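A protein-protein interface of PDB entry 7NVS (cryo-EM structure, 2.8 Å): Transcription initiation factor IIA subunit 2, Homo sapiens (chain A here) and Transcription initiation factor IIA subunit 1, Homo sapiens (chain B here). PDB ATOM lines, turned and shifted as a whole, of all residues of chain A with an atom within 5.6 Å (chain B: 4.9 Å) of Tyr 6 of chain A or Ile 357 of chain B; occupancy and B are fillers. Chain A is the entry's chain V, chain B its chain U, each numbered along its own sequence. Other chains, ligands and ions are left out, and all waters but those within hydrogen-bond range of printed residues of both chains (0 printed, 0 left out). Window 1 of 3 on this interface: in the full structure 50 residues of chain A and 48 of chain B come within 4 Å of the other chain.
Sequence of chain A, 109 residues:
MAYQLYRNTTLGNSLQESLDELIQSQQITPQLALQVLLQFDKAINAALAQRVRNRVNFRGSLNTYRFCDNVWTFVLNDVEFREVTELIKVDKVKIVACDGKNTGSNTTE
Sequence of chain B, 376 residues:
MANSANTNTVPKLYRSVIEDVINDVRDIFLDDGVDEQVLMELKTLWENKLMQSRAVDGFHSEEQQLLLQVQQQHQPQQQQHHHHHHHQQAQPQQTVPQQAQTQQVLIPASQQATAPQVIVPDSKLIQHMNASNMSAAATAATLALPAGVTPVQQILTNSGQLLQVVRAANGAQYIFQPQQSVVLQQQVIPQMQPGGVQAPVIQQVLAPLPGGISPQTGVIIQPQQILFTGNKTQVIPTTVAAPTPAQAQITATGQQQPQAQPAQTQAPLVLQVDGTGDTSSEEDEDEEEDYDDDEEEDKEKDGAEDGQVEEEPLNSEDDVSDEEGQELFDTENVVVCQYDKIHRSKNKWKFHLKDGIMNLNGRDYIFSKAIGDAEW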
ATOM      1  N   GLN A   4     -14.549   0.245 -13.719  1.00  0.00           N
ATOM      2  CA  GLN A   4     -14.055   1.622 -13.706  1.00  0.00           C
ATOM      3  C   GLN A   4     -12.593   1.692 -14.159  1.00  0.00           C
ATOM      4  O   GLN A   4     -11.695   2.076 -13.406  1.00  0.00           O
ATOM      5  CB  GLN A   4     -14.225   2.240 -12.314  1.00  0.00           C
ATOM      6  CG  GLN A   4     -15.633   2.132 -11.749  1.00  0.00           C
ATOM      7  CD  GLN A   4     -16.665   2.845 -12.598  1.00  0.00           C
ATOM      8  OE1 GLN A   4     -17.441   2.213 -13.313  1.00  0.00           O
ATOM      9  NE2 GLN A   4     -16.686   4.170 -12.516  1.00  0.00           N
ATOM     10  N   LEU A   5     -12.367   1.312 -15.417  1.00  0.00           N
ATOM     11  CA  LEU A   5     -11.034   1.332 -16.012  1.00  0.00           C
ATOM     12  C   LEU A   5     -10.801   2.542 -16.910  1.00  0.00           C
ATOM     13  O   LEU A   5      -9.804   3.251 -16.747  1.00  0.00           O
ATOM     14  CB  LEU A   5     -10.793   0.049 -16.815  1.00  0.00           C
ATOM     15  CG  LEU A   5     -10.175  -1.120 -16.048  1.00  0.00           C
ATOM     16  CD1 LEU A   5     -11.172  -1.694 -15.067  1.00  0.00           C
ATOM     17  CD2 LEU A   5      -9.685  -2.192 -17.009  1.00  0.00           C
ATOM     18  N   TYR A   6     -11.701   2.792 -17.858  1.00  0.00           N
ATOM     19  CA  TYR A   6     -11.492   3.807 -18.883  1.00  0.00           C
ATOM     20  C   TYR A   6     -11.861   5.210 -18.420  1.00  0.00           C
ATOM     21  O   TYR A   6     -11.867   6.136 -19.239  1.00  0.00           O
ATOM     22  CB  TYR A   6     -12.291   3.451 -20.140  1.00  0.00           C
ATOM     23  CG  TYR A   6     -12.209   1.990 -20.522  1.00  0.00           C
ATOM     24  CD1 TYR A   6     -11.146   1.507 -21.275  1.00  0.00           C
ATOM     25  CD2 TYR A   6     -13.195   1.094 -20.132  1.00  0.00           C
ATOM     26  CE1 TYR A   6     -11.067   0.172 -21.626  1.00  0.00           C
ATOM     27  CE2 TYR A   6     -13.125  -0.241 -20.477  1.00  0.00           C
ATOM     28  CZ  TYR A   6     -12.060  -0.697 -21.224  1.00  0.00           C
ATOM     29  OH  TYR A   6     -11.987  -2.027 -21.571  1.00  0.00           O
ATOM     30  N   ARG A   7     -12.172   5.394 -17.135  1.00  0.00           N
ATOM     31  CA  ARG A   7     -12.477   6.733 -16.642  1.00  0.00           C
ATOM     32  C   ARG A   7     -11.273   7.658 -16.773  1.00  0.00           C
ATOM     33  O   ARG A   7     -11.416   8.823 -17.162  1.00  0.00           O
ATOM     34  CB  ARG A   7     -12.941   6.665 -15.187  1.00  0.00           C
ATOM     35  CG  ARG A   7     -14.399   6.255 -15.021  1.00  0.00           C
ATOM     36  CD  ARG A   7     -14.924   6.576 -13.629  1.00  0.00           C
ATOM     37  NE  ARG A   7     -14.762   7.985 -13.280  1.00  0.00           N
ATOM     38  CZ  ARG A   7     -15.086   8.508 -12.102  1.00  0.00           C
ATOM     39  NH1 ARG A   7     -15.591   7.741 -11.144  1.00  0.00           N
ATOM     40  NH2 ARG A   7     -14.903   9.802 -11.877  1.00  0.00           N
ATOM     41  N   ASN A   8     -10.080   7.157 -16.457  1.00  0.00           N
ATOM     42  CA  ASN A   8      -8.860   7.963 -16.514  1.00  0.00           C
ATOM     43  C   ASN A   8      -8.254   7.919 -17.919  1.00  0.00           C
ATOM     44  O   ASN A   8      -7.133   7.465 -18.139  1.00  0.00           O
ATOM     45  CB  ASN A   8      -7.863   7.480 -15.466  1.00  0.00           C
ATOM     46  CG  ASN A   8      -6.724   8.458 -15.251  1.00  0.00           C
ATOM     47  OD1 ASN A   8      -5.699   8.392 -15.929  1.00  0.00           O
ATOM     48  ND2 ASN A   8      -6.900   9.372 -14.305  1.00  0.00           N
ATOM     49  N   THR A   9      -9.035   8.410 -18.881  1.00  0.00           N
ATOM     50  CA  THR A   9      -8.616   8.481 -20.273  1.00  0.00           C
ATOM     51  C   THR A   9      -9.167   9.763 -20.881  1.00  0.00           C
ATOM     52  O   THR A   9      -9.955  10.483 -20.259  1.00  0.00           O
ATOM     53  CB  THR A   9      -9.090   7.255 -21.065  1.00  0.00           C
ATOM     54  OG1 THR A   9     -10.522   7.242 -21.122  1.00  0.00           O
ATOM     55  CG2 THR A   9      -8.597   5.968 -20.418  1.00  0.00           C
ATOM     56  N   LEU A  11     -11.256   9.975 -23.400  1.00  0.00           N
ATOM     57  CA  LEU A  11     -12.696   9.786 -23.529  1.00  0.00           C
ATOM     58  C   LEU A  11     -13.385   9.936 -22.179  1.00  0.00           C
ATOM     59  O   LEU A  11     -14.418  10.606 -22.063  1.00  0.00           O
ATOM     60  CB  LEU A  11     -12.987   8.413 -24.136  1.00  0.00           C
ATOM     61  CG  LEU A  11     -14.452   7.973 -24.182  1.00  0.00           C
ATOM     62  CD1 LEU A  11     -15.338   9.071 -24.747  1.00  0.00           C
ATOM     63  CD2 LEU A  11     -14.596   6.695 -24.994  1.00  0.00           C
ATOM     64  N   GLY A  12     -12.820   9.321 -21.139  1.00  0.00           N
ATOM     65  CA  GLY A  12     -13.400   9.451 -19.813  1.00  0.00           C
ATOM     66  C   GLY A  12     -13.301  10.863 -19.270  1.00  0.00           C
ATOM     67  O   GLY A  12     -14.241  11.370 -18.651  1.00  0.00           O
ATOM     68  N   ASN A  13     -12.159  11.519 -19.492  1.00  0.00           N
ATOM     69  CA  ASN A  13     -11.982  12.880 -18.996  1.00  0.00           C
ATOM     70  C   ASN A  13     -12.987  13.832 -19.630  1.00  0.00           C
ATOM     71  O   ASN A  13     -13.558  14.690 -18.946  1.00  0.00           O
ATOM     72  CB  ASN A  13     -10.553  13.352 -19.265  1.00  0.00           C
ATOM     73  CG  ASN A  13     -10.211  14.629 -18.522  1.00  0.00           C
ATOM     74  OD1 ASN A  13     -11.064  15.230 -17.870  1.00  0.00           O
ATOM     75  ND2 ASN A  13      -8.955  15.050 -18.616  1.00  0.00           N
ATOM     76  N   ASP A  41     -19.525   3.314 -18.553  1.00  0.00           N
ATOM     77  CA  ASP A  41     -18.515   2.278 -18.374  1.00  0.00           C
ATOM     78  C   ASP A  41     -19.020   0.927 -18.866  1.00  0.00           C
ATOM     79  O   ASP A  41     -18.274   0.167 -19.494  1.00  0.00           O
ATOM     80  CB  ASP A  41     -18.104   2.197 -16.904  1.00  0.00           C
ATOM     81  CG  ASP A  41     -17.220   3.355 -16.482  1.00  0.00           C
ATOM     82  OD1 ASP A  41     -16.378   3.790 -17.296  1.00  0.00           O
ATOM     83  OD2 ASP A  41     -17.371   3.836 -15.340  1.00  0.00           O
ATOM     84  N   ILE A  44     -19.096   1.066 -22.855  1.00  0.00           N
ATOM     85  CA  ILE A  44     -17.780   0.982 -23.482  1.00  0.00           C
ATOM     86  C   ILE A  44     -17.182  -0.405 -23.283  1.00  0.00           C
ATOM     87  O   ILE A  44     -16.545  -0.956 -24.189  1.00  0.00           O
ATOM     88  CB  ILE A  44     -16.855   2.086 -22.938  1.00  0.00           C
ATOM     89  CG1 ILE A  44     -15.543   2.115 -23.725  1.00  0.00           C
ATOM     90  CG2 ILE A  44     -16.575   1.882 -21.458  1.00  0.00           C
ATOM     91  CD1 ILE A  44     -14.783   3.418 -23.593  1.00  0.00           C
ATOM     92  N   ASN A  45     -17.376  -0.994 -22.101  1.00  0.00           N
ATOM     93  CA  ASN A  45     -16.843  -2.327 -21.844  1.00  0.00           C
ATOM     94  C   ASN A  45     -17.437  -3.346 -22.807  1.00  0.00           C
ATOM     95  O   ASN A  45     -16.719  -4.182 -23.370  1.00  0.00           O
ATOM     96  CB  ASN A  45     -17.119  -2.732 -20.395  1.00  0.00           C
ATOM     97  CG  ASN A  45     -15.956  -2.426 -19.472  1.00  0.00           C
ATOM     98  OD1 ASN A  45     -14.973  -3.164 -19.428  1.00  0.00           O
ATOM     99  ND2 ASN A  45     -16.064  -1.332 -18.727  1.00  0.00           N
ATOM    100  N   LEU A  48     -16.090  -2.645 -26.513  1.00  0.00           N
ATOM    101  CA  LEU A  48     -14.728  -3.092 -26.783  1.00  0.00           C
ATOM    102  C   LEU A  48     -14.666  -4.603 -26.963  1.00  0.00           C
ATOM    103  O   LEU A  48     -13.986  -5.101 -27.867  1.00  0.00           O
ATOM    104  CB  LEU A  48     -13.799  -2.651 -25.652  1.00  0.00           C
ATOM    105  CG  LEU A  48     -13.039  -1.346 -25.899  1.00  0.00           C
ATOM    106  CD1 LEU A  48     -13.991  -0.160 -25.902  1.00  0.00           C
ATOM    107  CD2 LEU A  48     -11.949  -1.160 -24.856  1.00  0.00           C
ATOM    108  N   VAL B 334      -0.625   5.944 -21.697  1.00  0.00           N
ATOM    109  CA  VAL B 334      -1.210   4.987 -20.766  1.00  0.00           C
ATOM    110  C   VAL B 334      -1.998   3.957 -21.562  1.00  0.00           C
ATOM    111  O   VAL B 334      -2.707   4.303 -22.514  1.00  0.00           O
ATOM    112  CB  VAL B 334      -2.116   5.683 -19.729  1.00  0.00           C
ATOM    113  CG1 VAL B 334      -2.719   4.660 -18.776  1.00  0.00           C
ATOM    114  CG2 VAL B 334      -1.334   6.739 -18.963  1.00  0.00           C
ATOM    115  N   VAL B 335      -1.871   2.692 -21.169  1.00  0.00           N
ATOM    116  CA  VAL B 335      -2.535   1.579 -21.838  1.00  0.00           C
ATOM    117  C   VAL B 335      -3.473   0.918 -20.838  1.00  0.00           C
ATOM    118  O   VAL B 335      -3.054   0.558 -19.731  1.00  0.00           O
ATOM    119  CB  VAL B 335      -1.524   0.563 -22.393  1.00  0.00           C
ATOM    120  CG1 VAL B 335      -2.237  -0.700 -22.855  1.00  0.00           C
ATOM    121  CG2 VAL B 335      -0.723   1.177 -23.530  1.00  0.00           C
ATOM    122  N   VAL B 336      -4.734   0.761 -21.230  1.00  0.00           N
ATOM    123  CA  VAL B 336      -5.738   0.082 -20.421  1.00  0.00           C
ATOM    124  C   VAL B 336      -6.201  -1.153 -21.180  1.00  0.00           C
ATOM    125  O   VAL B 336      -6.578  -1.081 -22.355  1.00  0.00           O
ATOM    126  CB  VAL B 336      -6.928   1.005 -20.088  1.00  0.00           C
ATOM    127  CG1 VAL B 336      -7.901   0.305 -19.154  1.00  0.00           C
ATOM    128  CG2 VAL B 336      -6.436   2.308 -19.476  1.00  0.00           C
ATOM    129  N   CYS B 337      -6.172  -2.295 -20.498  1.00  0.00           N
ATOM    130  CA  CYS B 337      -6.411  -3.576 -21.151  1.00  0.00           C
ATOM    131  C   CYS B 337      -6.926  -4.569 -20.119  1.00  0.00           C
ATOM    132  O   CYS B 337      -7.097  -4.243 -18.941  1.00  0.00           O
ATOM    133  CB  CYS B 337      -5.136  -4.104 -21.810  1.00  0.00           C
ATOM    134  SG  CYS B 337      -3.804  -4.419 -20.626  1.00  0.00           S
ATOM    135  N   ASP B 355      -8.523  -7.867 -25.468  1.00  0.00           N
ATOM    136  CA  ASP B 355      -9.031  -6.581 -25.934  1.00  0.00           C
ATOM    137  C   ASP B 355      -8.747  -5.467 -24.935  1.00  0.00           C
ATOM    138  O   ASP B 355      -8.958  -5.624 -23.730  1.00  0.00           O
ATOM    139  CB  ASP B 355     -10.539  -6.678 -26.186  1.00  0.00           C
ATOM    140  CG  ASP B 355     -10.905  -7.819 -27.116  1.00  0.00           C
ATOM    141  OD1 ASP B 355     -10.768  -8.990 -26.704  1.00  0.00           O
ATOM    142  OD2 ASP B 355     -11.334  -7.544 -28.256  1.00  0.00           O
ATOM    143  N   GLY B 356      -8.268  -4.338 -25.450  1.00  0.00           N
ATOM    144  CA  GLY B 356      -7.936  -3.199 -24.619  1.00  0.00           C
ATOM    145  C   GLY B 356      -7.811  -1.952 -25.466  1.00  0.00           C
ATOM    146  O   GLY B 356      -8.006  -1.976 -26.683  1.00  0.00           O
ATOM    147  N   ILE B 357      -7.478  -0.846 -24.798  1.00  0.00           N
ATOM    148  CA  ILE B 357      -7.335   0.450 -25.444  1.00  0.00           C
ATOM    149  C   ILE B 357      -5.991   1.049 -25.055  1.00  0.00           C
ATOM    150  O   ILE B 357      -5.408   0.713 -24.021  1.00  0.00           O
ATOM    151  CB  ILE B 357      -8.485   1.413 -25.075  1.00  0.00           C
ATOM    152  CG1 ILE B 357      -8.577   2.554 -26.091  1.00  0.00           C
ATOM    153  CG2 ILE B 357      -8.291   1.963 -23.669  1.00  0.00           C
ATOM    154  CD1 ILE B 357      -9.867   3.340 -26.003  1.00  0.00           C
ATOM    155  N   MET B 358      -5.502   1.948 -25.907  1.00  0.00           N
ATOM    156  CA  MET B 358      -4.223   2.609 -25.694  1.00  0.00           C
ATOM    157  C   MET B 358      -4.338   4.070 -26.101  1.00  0.00           C
ATOM    158  O   MET B 358      -5.163   4.423 -26.949  1.00  0.00           O
ATOM    159  CB  MET B 358      -3.103   1.932 -26.495  1.00  0.00           C
ATOM    160  CG  MET B 358      -3.115   0.413 -26.418  1.00  0.00           C
ATOM    161  SD  MET B 358      -1.693  -0.342 -27.229  1.00  0.00           S
ATOM    162  CE  MET B 358      -2.209  -0.285 -28.942  1.00  0.00           C
ATOM    163  N   ASN B 359      -3.508   4.912 -25.491  1.00  0.00           N
ATOM    164  CA  ASN B 359      -3.447   6.341 -25.785  1.00  0.00           C
ATOM    165  C   ASN B 359      -1.984   6.692 -26.039  1.00  0.00           C
ATOM    166  O   ASN B 359      -1.260   7.082 -25.120  1.00  0.00           O
ATOM    167  CB  ASN B 359      -4.037   7.166 -24.640  1.00  0.00           C
ATOM    168  CG  ASN B 359      -4.136   8.641 -24.976  1.00  0.00           C
ATOM    169  OD1 ASN B 359      -3.797   9.063 -26.081  1.00  0.00           O
ATOM    170  ND2 ASN B 359      -4.604   9.435 -24.019  1.00  0.00           N
ATOM    171  N   ASP B 364      -5.582   7.532 -30.226  1.00  0.00           N
ATOM    172  CA  ASP B 364      -6.251   6.441 -29.530  1.00  0.00           C
ATOM    173  C   ASP B 364      -6.154   5.177 -30.377  1.00  0.00           C
ATOM    174  O   ASP B 364      -6.550   5.177 -31.548  1.00  0.00           O
ATOM    175  CB  ASP B 364      -7.713   6.791 -29.252  1.00  0.00           C
ATOM    176  CG  ASP B 364      -8.407   5.753 -28.394  1.00  0.00           C
ATOM    177  OD1 ASP B 364      -8.009   5.588 -27.220  1.00  0.00           O
ATOM    178  OD2 ASP B 364      -9.350   5.102 -28.892  1.00  0.00           O
ATOM    179  N   TYR B 365      -5.630   4.109 -29.783  1.00  0.00           N
ATOM    180  CA  TYR B 365      -5.488   2.823 -30.446  1.00  0.00           C
ATOM    181  C   TYR B 365      -6.275   1.760 -29.694  1.00  0.00           C
ATOM    182  O   TYR B 365      -6.268   1.713 -28.461  1.00  0.00           O
ATOM    183  CB  TYR B 365      -4.015   2.410 -30.537  1.00  0.00           C
ATOM    184  CG  TYR B 365      -3.206   3.234 -31.512  1.00  0.00           C
ATOM    185  CD1 TYR B 365      -3.379   3.093 -32.882  1.00  0.00           C
ATOM    186  CD2 TYR B 365      -2.266   4.153 -31.062  1.00  0.00           C
ATOM    187  CE1 TYR B 365      -2.640   3.844 -33.777  1.00  0.00           C
ATOM    188  CE2 TYR B 365      -1.524   4.908 -31.949  1.00  0.00           C
ATOM    189  CZ  TYR B 365      -1.714   4.749 -33.305  1.00  0.00           C
ATOM    190  OH  TYR B 365      -0.977   5.499 -34.192  1.00  0.00           O
ATOM    191  N   ILE B 366      -6.957   0.903 -30.452  1.00  0.00           N
ATOM    192  CA  ILE B 366      -7.769  -0.172 -29.899  1.00  0.00           C
ATOM    193  C   ILE B 366      -7.317  -1.489 -30.513  1.00  0.00           C
ATOM    194  O   ILE B 366      -7.107  -1.580 -31.727  1.00  0.00           O
ATOM    195  CB  ILE B 366      -9.274   0.063 -30.151  1.00  0.00           C
ATOM    196  CG1 ILE B 366     -10.112  -0.795 -29.201  1.00  0.00           C
ATOM    197  CG2 ILE B 366      -9.634  -0.242 -31.599  1.00  0.00           C
ATOM    198  CD1 ILE B 366     -10.201  -0.240 -27.795  1.00  0.00           C
ATOM    199  N   PHE B 367      -7.160  -2.506 -29.668  1.00  0.00           N
ATOM    200  CA  PHE B 367      -6.724  -3.825 -30.098  1.00  0.00           C
ATOM    201  C   PHE B 367      -7.595  -4.883 -29.437  1.00  0.00           C
ATOM    202  O   PHE B 367      -8.179  -4.662 -28.373  1.00  0.00           O
ATOM    203  CB  PHE B 367      -5.249  -4.070 -29.752  1.00  0.00           C
ATOM    204  CG  PHE B 367      -4.951  -3.991 -28.283  1.00  0.00           C
ATOM    205  CD1 PHE B 367      -4.728  -2.768 -27.672  1.00  0.00           C
ATOM    206  CD2 PHE B 367      -4.894  -5.140 -27.512  1.00  0.00           C
ATOM    207  CE1 PHE B 367      -4.454  -2.693 -26.320  1.00  0.00           C
ATOM    208  CE2 PHE B 367      -4.621  -5.071 -26.159  1.00  0.00           C
ATOM    209  CZ  PHE B 367      -4.401  -3.846 -25.563  1.00  0.00           C
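Leu 5 of chain A touches Val 336 of chain B (CB to CG1, 3.7 Å).
Cys 337 of chain B touches Leu 5 of chain A (O to CD2, 3.8 Å).
Tyr 6 of chain A touches Ile 357 of chain B.
Leu 48 of chain A touches Asp 355 of chain B (O to OD2, 3.6 Å).
Ile 366 of chain B touches Leu 48 of chain A.
O of Val 336 of chain B sits at hydrogen-bond distance from N of Ile 357 of chain B, 2.6 Å away.
The backbone carbonyl oxygen of Tyr 6 of chain A is in hydrogen-bond range of the side-chain hydroxyl of Thr 9 of chain A.
Of the 13 printed residues of chain A, 3 touch a printed residue of chain B.
Among the printed residues, 5 pairs touch across the chains.
Among the printed residues, no Asp or Glu carboxylate lies within 4 Å of a Lys or Arg side-chain nitrogen of the other chain.
Printed residues of chain B within 4 Å of Tyr 6 of chain A: Ile 357 (3.8 Å).
Of chain A, only Tyr 6 (3.8 Å) comes within 4 Å of Ile 357 of chain B.
Of the printed residues of chain A, Ile 366 of chain B touches Leu 48.
Printed residues of chain A within 4 Å of Val 336 of chain B: Leu 5.
Printed residues of chain B within 4 Å of Leu 48 of chain A: Asp 355 (3.6 Å) and Ile 366 (3.5 Å).
The nearest residue of chain A that does not touch Ile 357 of chain B is Leu 48 of chain A (4.3 Å).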
